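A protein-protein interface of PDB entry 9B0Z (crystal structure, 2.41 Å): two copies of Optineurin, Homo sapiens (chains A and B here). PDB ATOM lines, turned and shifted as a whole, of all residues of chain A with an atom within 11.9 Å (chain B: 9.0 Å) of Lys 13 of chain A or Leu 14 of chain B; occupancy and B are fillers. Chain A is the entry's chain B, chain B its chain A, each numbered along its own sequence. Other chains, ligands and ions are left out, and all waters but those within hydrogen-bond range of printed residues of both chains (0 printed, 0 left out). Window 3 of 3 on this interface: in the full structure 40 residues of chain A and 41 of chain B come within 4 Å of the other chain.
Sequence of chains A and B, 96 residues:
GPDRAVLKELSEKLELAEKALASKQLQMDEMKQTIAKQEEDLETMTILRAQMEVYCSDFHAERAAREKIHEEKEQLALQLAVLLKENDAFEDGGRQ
Of chain B, only Leu 14 (3.5 Å) and Glu 18 (3.6 Å) come within 4 Å of Lys 13 of chain A. Of chain A, only Lys 13 (3.5 Å) and Leu 14 (3.5 Å) come within 4 Å of Leu 14 of chain B. No residue of chain B comes within 4 Å of Glu 12 of chain A. No residue of chain A comes within 4 Å of Leu 10 of chain B. No residue of chain A comes within 4 Å of Ser 11 of chain B. Of chain A, only Leu 14 comes within 4 Å of Lys 13 of chain B. No residue of chain A comes within 4 Å of Glu 15 of chain B. Glu 18 of chain B touches just one residue of chain A: Lys 13 (3.6 Å). Printed residues of chain B within 4 Å of Leu 14 of chain A: Lys 13 and Leu 14. Of the printed residues of chain B, Leu 7 of chain A touches Leu 7. Of the printed residues of chain A, Ala 20 of chain B touches Leu 21. Ala 17 of chain B touches none of the printed residues of chain A. Lys 19 of chain B touches none of the printed residues of chain A.
OE2 of Glu 18 of chain B lies within salt-bridge range of NZ of Lys 13 of chain A.
Among the printed residues, pairs that only touch across the chains: Leu 14 of chain A with Leu 14 of chain B, Leu 7 of chain A with Leu 7 of chain B, Lys 13 of chain A with Leu 14 of chain B, Leu 21 of chain A with Leu 21 of chain B, Leu 14 of chain A with Lys 13 of chain B, Leu 21 of chain A with Ala 20 of chain B and Ala 20 of chain A with Leu 21 of chain B.
Of the 19 printed residues of chain A, 5 touch a printed residue of chain B. Printed residues of chain A that touch a printed residue of chain B: Leu 7, Lys 13, Leu 14, Ala 20 and Leu 21. Hydrophobic or aromatic side chains of chain A that line the printed part of chain B: Leu 7, Leu 14, Ala 20 and Leu 21. Hydrophobic or aromatic side chains of chain B within 4 Å of the printed part of chain A: Leu 7, Leu 14 and Leu 21.
Leu 7 of chain A touches its own counterpart, Leu 7 of chain B. Lys 13 of chain A touches Leu 14 of chain B, and with the chains exchanged Leu 14 of chain A touches Lys 13 of chain B. Lys 13 of chain A touches Glu 18 of chain B, but with the chains exchanged Glu 18 of chain A does not touch Lys 13 of chain B (7.6 Å). Leu 21 of chain A touches its own counterpart, Leu 21 of chain B. 16 positions are printed for both chains. Of the 8 pairs that touch across the chains among the printed residues, 7 have their exchanged pair printed and touching as well.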
ATOM      1  N   ARG A   4      -8.324  13.848 -27.888  1.00  0.00           N
ATOM      2  CA  ARG A   4      -8.990  13.439 -26.652  1.00  0.00           C
ATOM      3  C   ARG A   4      -8.443  12.110 -26.144  1.00  0.00           C
ATOM      4  O   ARG A   4      -8.178  11.948 -24.946  1.00  0.00           O
ATOM      5  CB  ARG A   4     -10.499  13.353 -26.872  1.00  0.00           C
ATOM      6  N   ALA A   5      -8.278  11.138 -27.047  1.00  0.00           N
ATOM      7  CA  ALA A   5      -7.785   9.825 -26.643  1.00  0.00           C
ATOM      8  C   ALA A   5      -6.370   9.915 -26.086  1.00  0.00           C
ATOM      9  O   ALA A   5      -6.025   9.202 -25.134  1.00  0.00           O
ATOM     10  CB  ALA A   5      -7.842   8.854 -27.820  1.00  0.00           C
ATOM     11  N   VAL A   6      -5.530  10.775 -26.673  1.00  0.00           N
ATOM     12  CA  VAL A   6      -4.156  10.917 -26.199  1.00  0.00           C
ATOM     13  C   VAL A   6      -4.138  11.413 -24.761  1.00  0.00           C
ATOM     14  O   VAL A   6      -3.213  11.103 -24.000  1.00  0.00           O
ATOM     15  CB  VAL A   6      -3.355  11.850 -27.128  1.00  0.00           C
ATOM     16  N   LEU A   7      -5.143  12.193 -24.362  1.00  0.00           N
ATOM     17  CA  LEU A   7      -5.241  12.627 -22.976  1.00  0.00           C
ATOM     18  C   LEU A   7      -5.928  11.601 -22.087  1.00  0.00           C
ATOM     19  O   LEU A   7      -5.719  11.626 -20.868  1.00  0.00           O
ATOM     20  CB  LEU A   7      -5.956  13.975 -22.869  1.00  0.00           C
ATOM     21  CG  LEU A   7      -4.923  15.040 -22.495  1.00  0.00           C
ATOM     22  CD1 LEU A   7      -4.009  15.311 -23.685  1.00  0.00           C
ATOM     23  CD2 LEU A   7      -5.565  16.320 -21.971  1.00  0.00           C
ATOM     24  N   LYS A   8      -6.736  10.705 -22.659  1.00  0.00           N
ATOM     25  CA  LYS A   8      -7.162   9.533 -21.901  1.00  0.00           C
ATOM     26  C   LYS A   8      -5.947   8.765 -21.404  1.00  0.00           C
ATOM     27  O   LYS A   8      -5.946   8.244 -20.282  1.00  0.00           O
ATOM     28  CB  LYS A   8      -8.060   8.634 -22.754  1.00  0.00           C
ATOM     29  N   GLU A   9      -4.908   8.679 -22.238  1.00  0.00           N
ATOM     30  CA  GLU A   9      -3.665   8.034 -21.833  1.00  0.00           C
ATOM     31  C   GLU A   9      -3.058   8.731 -20.619  1.00  0.00           C
ATOM     32  O   GLU A   9      -2.829   8.108 -19.575  1.00  0.00           O
ATOM     33  CB  GLU A   9      -2.667   8.046 -22.991  1.00  0.00           C
ATOM     34  CG  GLU A   9      -2.918   7.022 -24.079  1.00  0.00           C
ATOM     35  CD  GLU A   9      -1.667   6.747 -24.897  1.00  0.00           C
ATOM     36  OE1 GLU A   9      -0.906   7.702 -25.164  1.00  0.00           O
ATOM     37  OE2 GLU A   9      -1.432   5.572 -25.253  1.00  0.00           O
ATOM     38  N   LEU A  10      -2.783  10.033 -20.749  1.00  0.00           N
ATOM     39  CA  LEU A  10      -2.141  10.778 -19.668  1.00  0.00           C
ATOM     40  C   LEU A  10      -3.003  10.803 -18.408  1.00  0.00           C
ATOM     41  O   LEU A  10      -2.486  10.687 -17.292  1.00  0.00           O
ATOM     42  CB  LEU A  10      -1.816  12.195 -20.133  1.00  0.00           C
ATOM     43  CG  LEU A  10      -0.824  12.256 -21.296  1.00  0.00           C
ATOM     44  CD1 LEU A  10      -0.336  13.678 -21.525  1.00  0.00           C
ATOM     45  CD2 LEU A  10       0.349  11.320 -21.044  1.00  0.00           C
ATOM     46  N   SER A  11      -4.318  10.970 -18.567  1.00  0.00           N
ATOM     47  CA  SER A  11      -5.223  10.942 -17.422  1.00  0.00           C
ATOM     48  C   SER A  11      -5.077   9.642 -16.634  1.00  0.00           C
ATOM     49  O   SER A  11      -4.878   9.657 -15.412  1.00  0.00           O
ATOM     50  CB  SER A  11      -6.663  11.134 -17.905  1.00  0.00           C
ATOM     51  OG  SER A  11      -7.605  10.608 -16.986  1.00  0.00           O
ATOM     52  N   GLU A  12      -5.164   8.503 -17.324  1.00  0.00           N
ATOM     53  CA  GLU A  12      -5.119   7.211 -16.644  1.00  0.00           C
ATOM     54  C   GLU A  12      -3.765   6.960 -15.989  1.00  0.00           C
ATOM     55  O   GLU A  12      -3.695   6.355 -14.912  1.00  0.00           O
ATOM     56  CB  GLU A  12      -5.447   6.097 -17.636  1.00  0.00           C
ATOM     57  N   LYS A  13      -2.680   7.396 -16.631  1.00  0.00           N
ATOM     58  CA  LYS A  13      -1.347   7.190 -16.074  1.00  0.00           C
ATOM     59  C   LYS A  13      -1.113   8.048 -14.833  1.00  0.00           C
ATOM     60  O   LYS A  13      -0.603   7.555 -13.819  1.00  0.00           O
ATOM     61  CB  LYS A  13      -0.295   7.476 -17.142  1.00  0.00           C
ATOM     62  CG  LYS A  13       0.867   6.504 -17.145  1.00  0.00           C
ATOM     63  CD  LYS A  13       2.110   7.165 -17.716  1.00  0.00           C
ATOM     64  CE  LYS A  13       3.227   6.165 -17.962  1.00  0.00           C
ATOM     65  NZ  LYS A  13       4.249   6.709 -18.905  1.00  0.00           N
ATOM     66  N   LEU A  14      -1.498   9.326 -14.889  1.00  0.00           N
ATOM     67  CA  LEU A  14      -1.355  10.201 -13.729  1.00  0.00           C
ATOM     68  C   LEU A  14      -2.072   9.636 -12.514  1.00  0.00           C
ATOM     69  O   LEU A  14      -1.540   9.672 -11.401  1.00  0.00           O
ATOM     70  CB  LEU A  14      -1.884  11.591 -14.061  1.00  0.00           C
ATOM     71  CG  LEU A  14      -1.259  12.754 -13.299  1.00  0.00           C
ATOM     72  CD1 LEU A  14       0.221  12.872 -13.595  1.00  0.00           C
ATOM     73  CD2 LEU A  14      -1.973  14.032 -13.696  1.00  0.00           C
ATOM     74  N   GLU A  15      -3.284   9.113 -12.701  1.00  0.00           N
ATOM     75  CA  GLU A  15      -3.982   8.497 -11.579  1.00  0.00           C
ATOM     76  C   GLU A  15      -3.243   7.254 -11.106  1.00  0.00           C
ATOM     77  O   GLU A  15      -3.150   7.005  -9.899  1.00  0.00           O
ATOM     78  CB  GLU A  15      -5.422   8.156 -11.961  1.00  0.00           C
ATOM     79  N   LEU A  16      -2.696   6.472 -12.040  1.00  0.00           N
ATOM     80  CA  LEU A  16      -1.945   5.281 -11.652  1.00  0.00           C
ATOM     81  C   LEU A  16      -0.680   5.654 -10.894  1.00  0.00           C
ATOM     82  O   LEU A  16      -0.358   5.039  -9.869  1.00  0.00           O
ATOM     83  CB  LEU A  16      -1.603   4.451 -12.889  1.00  0.00           C
ATOM     84  CG  LEU A  16      -1.441   2.942 -12.697  1.00  0.00           C
ATOM     85  CD1 LEU A  16      -2.751   2.297 -12.241  1.00  0.00           C
ATOM     86  CD2 LEU A  16      -0.956   2.322 -13.996  1.00  0.00           C
ATOM     87  N   ALA A  17       0.035   6.677 -11.365  1.00  0.00           N
ATOM     88  CA  ALA A  17       1.246   7.109 -10.677  1.00  0.00           C
ATOM     89  C   ALA A  17       0.922   7.697  -9.308  1.00  0.00           C
ATOM     90  O   ALA A  17       1.628   7.433  -8.329  1.00  0.00           O
ATOM     91  CB  ALA A  17       2.009   8.119 -11.535  1.00  0.00           C
ATOM     92  N   GLU A  18      -0.146   8.491  -9.216  1.00  0.00           N
ATOM     93  CA  GLU A  18      -0.508   9.073  -7.929  1.00  0.00           C
ATOM     94  C   GLU A  18      -0.937   7.997  -6.938  1.00  0.00           C
ATOM     95  O   GLU A  18      -0.648   8.097  -5.739  1.00  0.00           O
ATOM     96  CB  GLU A  18      -1.610  10.114  -8.119  1.00  0.00           C
ATOM     97  N   LYS A  19      -1.617   6.951  -7.418  1.00  0.00           N
ATOM     98  CA  LYS A  19      -1.957   5.829  -6.549  1.00  0.00           C
ATOM     99  C   LYS A  19      -0.705   5.095  -6.084  1.00  0.00           C
ATOM    100  O   LYS A  19      -0.602   4.709  -4.912  1.00  0.00           O
ATOM    101  CB  LYS A  19      -2.911   4.873  -7.264  1.00  0.00           C
ATOM    102  N   ALA A  20       0.256   4.892  -6.989  1.00  0.00           N
ATOM    103  CA  ALA A  20       1.503   4.229  -6.613  1.00  0.00           C
ATOM    104  C   ALA A  20       2.262   5.025  -5.559  1.00  0.00           C
ATOM    105  O   ALA A  20       2.761   4.456  -4.580  1.00  0.00           O
ATOM    106  CB  ALA A  20       2.370   4.016  -7.851  1.00  0.00           C
ATOM    107  N   LEU A  21       2.351   6.346  -5.734  1.00  0.00           N
ATOM    108  CA  LEU A  21       2.966   7.192  -4.711  1.00  0.00           C
ATOM    109  C   LEU A  21       2.314   6.970  -3.357  1.00  0.00           C
ATOM    110  O   LEU A  21       2.998   6.869  -2.336  1.00  0.00           O
ATOM    111  CB  LEU A  21       2.859   8.663  -5.117  1.00  0.00           C
ATOM    112  CG  LEU A  21       4.011   9.212  -5.958  1.00  0.00           C
ATOM    113  CD1 LEU A  21       3.828  10.689  -6.207  1.00  0.00           C
ATOM    114  CD2 LEU A  21       5.342   8.958  -5.272  1.00  0.00           C
ATOM    115  N   ALA A  22       0.982   6.911  -3.332  1.00  0.00           N
ATOM    116  CA  ALA A  22       0.270   6.636  -2.090  1.00  0.00           C
ATOM    117  C   ALA A  22       0.683   5.292  -1.515  1.00  0.00           C
ATOM    118  O   ALA A  22       0.969   5.176  -0.318  1.00  0.00           O
ATOM    119  CB  ALA A  22      -1.235   6.679  -2.336  1.00  0.00           C
ATOM    120  N   LEU B   7      -2.414  19.676 -22.196  1.00  0.00           N
ATOM    121  CA  LEU B   7      -1.591  18.489 -22.369  1.00  0.00           C
ATOM    122  C   LEU B   7      -0.131  18.765 -22.048  1.00  0.00           C
ATOM    123  O   LEU B   7       0.593  17.843 -21.657  1.00  0.00           O
ATOM    124  CB  LEU B   7      -1.723  17.957 -23.798  1.00  0.00           C
ATOM    125  N   LYS B   8       0.326  20.008 -22.214  1.00  0.00           N
ATOM    126  CA  LYS B   8       1.621  20.387 -21.662  1.00  0.00           C
ATOM    127  C   LYS B   8       1.613  20.286 -20.142  1.00  0.00           C
ATOM    128  O   LYS B   8       2.528  19.715 -19.540  1.00  0.00           O
ATOM    129  CB  LYS B   8       1.987  21.804 -22.102  1.00  0.00           C
ATOM    130  N   GLU B   9       0.552  20.794 -19.511  1.00  0.00           N
ATOM    131  CA  GLU B   9       0.442  20.767 -18.054  1.00  0.00           C
ATOM    132  C   GLU B   9       0.453  19.339 -17.524  1.00  0.00           C
ATOM    133  O   GLU B   9       1.277  18.983 -16.675  1.00  0.00           O
ATOM    134  CB  GLU B   9      -0.828  21.498 -17.615  1.00  0.00           C
ATOM    135  N   LEU B  10      -0.464  18.504 -18.020  1.00  0.00           N
ATOM    136  CA  LEU B  10      -0.554  17.135 -17.527  1.00  0.00           C
ATOM    137  C   LEU B  10       0.757  16.385 -17.738  1.00  0.00           C
ATOM    138  O   LEU B  10       1.198  15.638 -16.859  1.00  0.00           O
ATOM    139  CB  LEU B  10      -1.709  16.406 -18.213  1.00  0.00           C
ATOM    140  N   SER B  11       1.406  16.594 -18.890  1.00  0.00           N
ATOM    141  CA  SER B  11       2.694  15.955 -19.166  1.00  0.00           C
ATOM    142  C   SER B  11       3.714  16.259 -18.079  1.00  0.00           C
ATOM    143  O   SER B  11       4.350  15.349 -17.534  1.00  0.00           O
ATOM    144  CB  SER B  11       3.225  16.407 -20.524  1.00  0.00           C
ATOM    145  N   GLU B  12       3.894  17.540 -17.761  1.00  0.00           N
ATOM    146  CA  GLU B  12       4.905  17.932 -16.784  1.00  0.00           C
ATOM    147  C   GLU B  12       4.590  17.377 -15.398  1.00  0.00           C
ATOM    148  O   GLU B  12       5.508  17.069 -14.628  1.00  0.00           O
ATOM    149  CB  GLU B  12       5.042  19.453 -16.778  1.00  0.00           C
ATOM    150  CG  GLU B  12       5.025  20.034 -18.192  1.00  0.00           C
ATOM    151  CD  GLU B  12       5.504  21.470 -18.286  1.00  0.00           C
ATOM    152  OE1 GLU B  12       6.491  21.709 -19.014  1.00  0.00           O
ATOM    153  OE2 GLU B  12       4.900  22.356 -17.644  1.00  0.00           O
ATOM    154  N   LYS B  13       3.303  17.252 -15.058  1.00  0.00           N
ATOM    155  CA  LYS B  13       2.933  16.664 -13.773  1.00  0.00           C
ATOM    156  C   LYS B  13       3.298  15.183 -13.725  1.00  0.00           C
ATOM    157  O   LYS B  13       3.811  14.698 -12.708  1.00  0.00           O
ATOM    158  CB  LYS B  13       1.443  16.860 -13.515  1.00  0.00           C
ATOM    159  CG  LYS B  13       1.127  17.233 -12.082  1.00  0.00           C
ATOM    160  CD  LYS B  13      -0.271  16.798 -11.677  1.00  0.00           C
ATOM    161  CE  LYS B  13      -0.634  17.418 -10.335  1.00  0.00           C
ATOM    162  NZ  LYS B  13      -2.100  17.446 -10.077  1.00  0.00           N
ATOM    163  N   LEU B  14       3.038  14.450 -14.815  1.00  0.00           N
ATOM    164  CA  LEU B  14       3.455  13.052 -14.886  1.00  0.00           C
ATOM    165  C   LEU B  14       4.945  12.915 -14.636  1.00  0.00           C
ATOM    166  O   LEU B  14       5.378  12.044 -13.876  1.00  0.00           O
ATOM    167  CB  LEU B  14       3.122  12.473 -16.262  1.00  0.00           C
ATOM    168  CG  LEU B  14       2.933  10.960 -16.415  1.00  0.00           C
ATOM    169  CD1 LEU B  14       1.719  10.436 -15.667  1.00  0.00           C
ATOM    170  CD2 LEU B  14       2.867  10.616 -17.900  1.00  0.00           C
ATOM    171  N   GLU B  15       5.746  13.792 -15.246  1.00  0.00           N
ATOM    172  CA  GLU B  15       7.184  13.733 -15.025  1.00  0.00           C
ATOM    173  C   GLU B  15       7.522  14.048 -13.578  1.00  0.00           C
ATOM    174  O   GLU B  15       8.421  13.432 -12.999  1.00  0.00           O
ATOM    175  CB  GLU B  15       7.912  14.681 -15.976  1.00  0.00           C
ATOM    176  CG  GLU B  15       9.431  14.452 -16.045  1.00  0.00           C
ATOM    177  CD  GLU B  15       9.813  13.077 -16.609  1.00  0.00           C
ATOM    178  OE1 GLU B  15       8.910  12.347 -17.077  1.00  0.00           O
ATOM    179  OE2 GLU B  15      11.015  12.726 -16.593  1.00  0.00           O
ATOM    180  N   LEU B  16       6.815  15.005 -12.974  1.00  0.00           N
ATOM    181  CA  LEU B  16       7.061  15.288 -11.565  1.00  0.00           C
ATOM    182  C   LEU B  16       6.662  14.101 -10.697  1.00  0.00           C
ATOM    183  O   LEU B  16       7.379  13.744  -9.756  1.00  0.00           O
ATOM    184  CB  LEU B  16       6.312  16.549 -11.132  1.00  0.00           C
ATOM    185  N   ALA B  17       5.533  13.464 -11.014  1.00  0.00           N
ATOM    186  CA  ALA B  17       5.082  12.334 -10.208  1.00  0.00           C
ATOM    187  C   ALA B  17       6.041  11.156 -10.324  1.00  0.00           C
ATOM    188  O   ALA B  17       6.360  10.502  -9.323  1.00  0.00           O
ATOM    189  CB  ALA B  17       3.669  11.926 -10.624  1.00  0.00           C
ATOM    190  N   GLU B  18       6.507  10.866 -11.533  1.00  0.00           N
ATOM    191  CA  GLU B  18       7.443   9.765 -11.712  1.00  0.00           C
ATOM    192  C   GLU B  18       8.804  10.066 -11.096  1.00  0.00           C
ATOM    193  O   GLU B  18       9.491   9.147 -10.631  1.00  0.00           O
ATOM    194  CB  GLU B  18       7.538   9.424 -13.188  1.00  0.00           C
ATOM    195  CG  GLU B  18       6.234   8.855 -13.706  1.00  0.00           C
ATOM    196  CD  GLU B  18       6.366   8.337 -15.104  1.00  0.00           C
ATOM    197  OE1 GLU B  18       7.357   8.714 -15.761  1.00  0.00           O
ATOM    198  OE2 GLU B  18       5.504   7.546 -15.543  1.00  0.00           O
ATOM    199  N   LYS B  19       9.226  11.332 -11.106  1.00  0.00           N
ATOM    200  CA  LYS B  19      10.445  11.700 -10.394  1.00  0.00           C
ATOM    201  C   LYS B  19      10.280  11.504  -8.889  1.00  0.00           C
ATOM    202  O   LYS B  19      11.191  11.003  -8.218  1.00  0.00           O
ATOM    203  CB  LYS B  19      10.836  13.140 -10.723  1.00  0.00           C
ATOM    204  CG  LYS B  19      11.394  13.308 -12.136  1.00  0.00           C
ATOM    205  CD  LYS B  19      12.329  14.500 -12.243  1.00  0.00           C
ATOM    206  CE  LYS B  19      13.258  14.361 -13.445  1.00  0.00           C
ATOM    207  NZ  LYS B  19      14.387  15.335 -13.391  1.00  0.00           N
ATOM    208  N   ALA B  20       9.124  11.894  -8.342  1.00  0.00           N
ATOM    209  CA  ALA B  20       8.868  11.669  -6.921  1.00  0.00           C
ATOM    210  C   ALA B  20       8.840  10.178  -6.596  1.00  0.00           C
ATOM    211  O   ALA B  20       9.402   9.749  -5.580  1.00  0.00           O
ATOM    212  CB  ALA B  20       7.557  12.337  -6.506  1.00  0.00           C
ATOM    213  N   LEU B  21       8.197   9.374  -7.451  1.00  0.00           N
ATOM    214  CA  LEU B  21       8.211   7.923  -7.272  1.00  0.00           C
ATOM    215  C   LEU B  21       9.634   7.402  -7.144  1.00  0.00           C
ATOM    216  O   LEU B  21       9.939   6.614  -6.247  1.00  0.00           O
ATOM    217  CB  LEU B  21       7.504   7.248  -8.450  1.00  0.00           C
ATOM    218  CG  LEU B  21       6.010   6.940  -8.397  1.00  0.00           C
ATOM    219  CD1 LEU B  21       5.605   6.243  -9.663  1.00  0.00           C
ATOM    220  CD2 LEU B  21       5.754   6.010  -7.234  1.00  0.00           C
ATOM    221  N   ALA B  22      10.523   7.842  -8.035  1.00  0.00           N
ATOM    222  CA  ALA B  22      11.927   7.463  -7.925  1.00  0.00           C
ATOM    223  C   ALA B  22      12.514   7.939  -6.604  1.00  0.00           C
ATOM    224  O   ALA B  22      13.158   7.169  -5.880  1.00  0.00           O
ATOM    225  CB  ALA B  22      12.718   8.033  -9.102  1.00  0.00           C
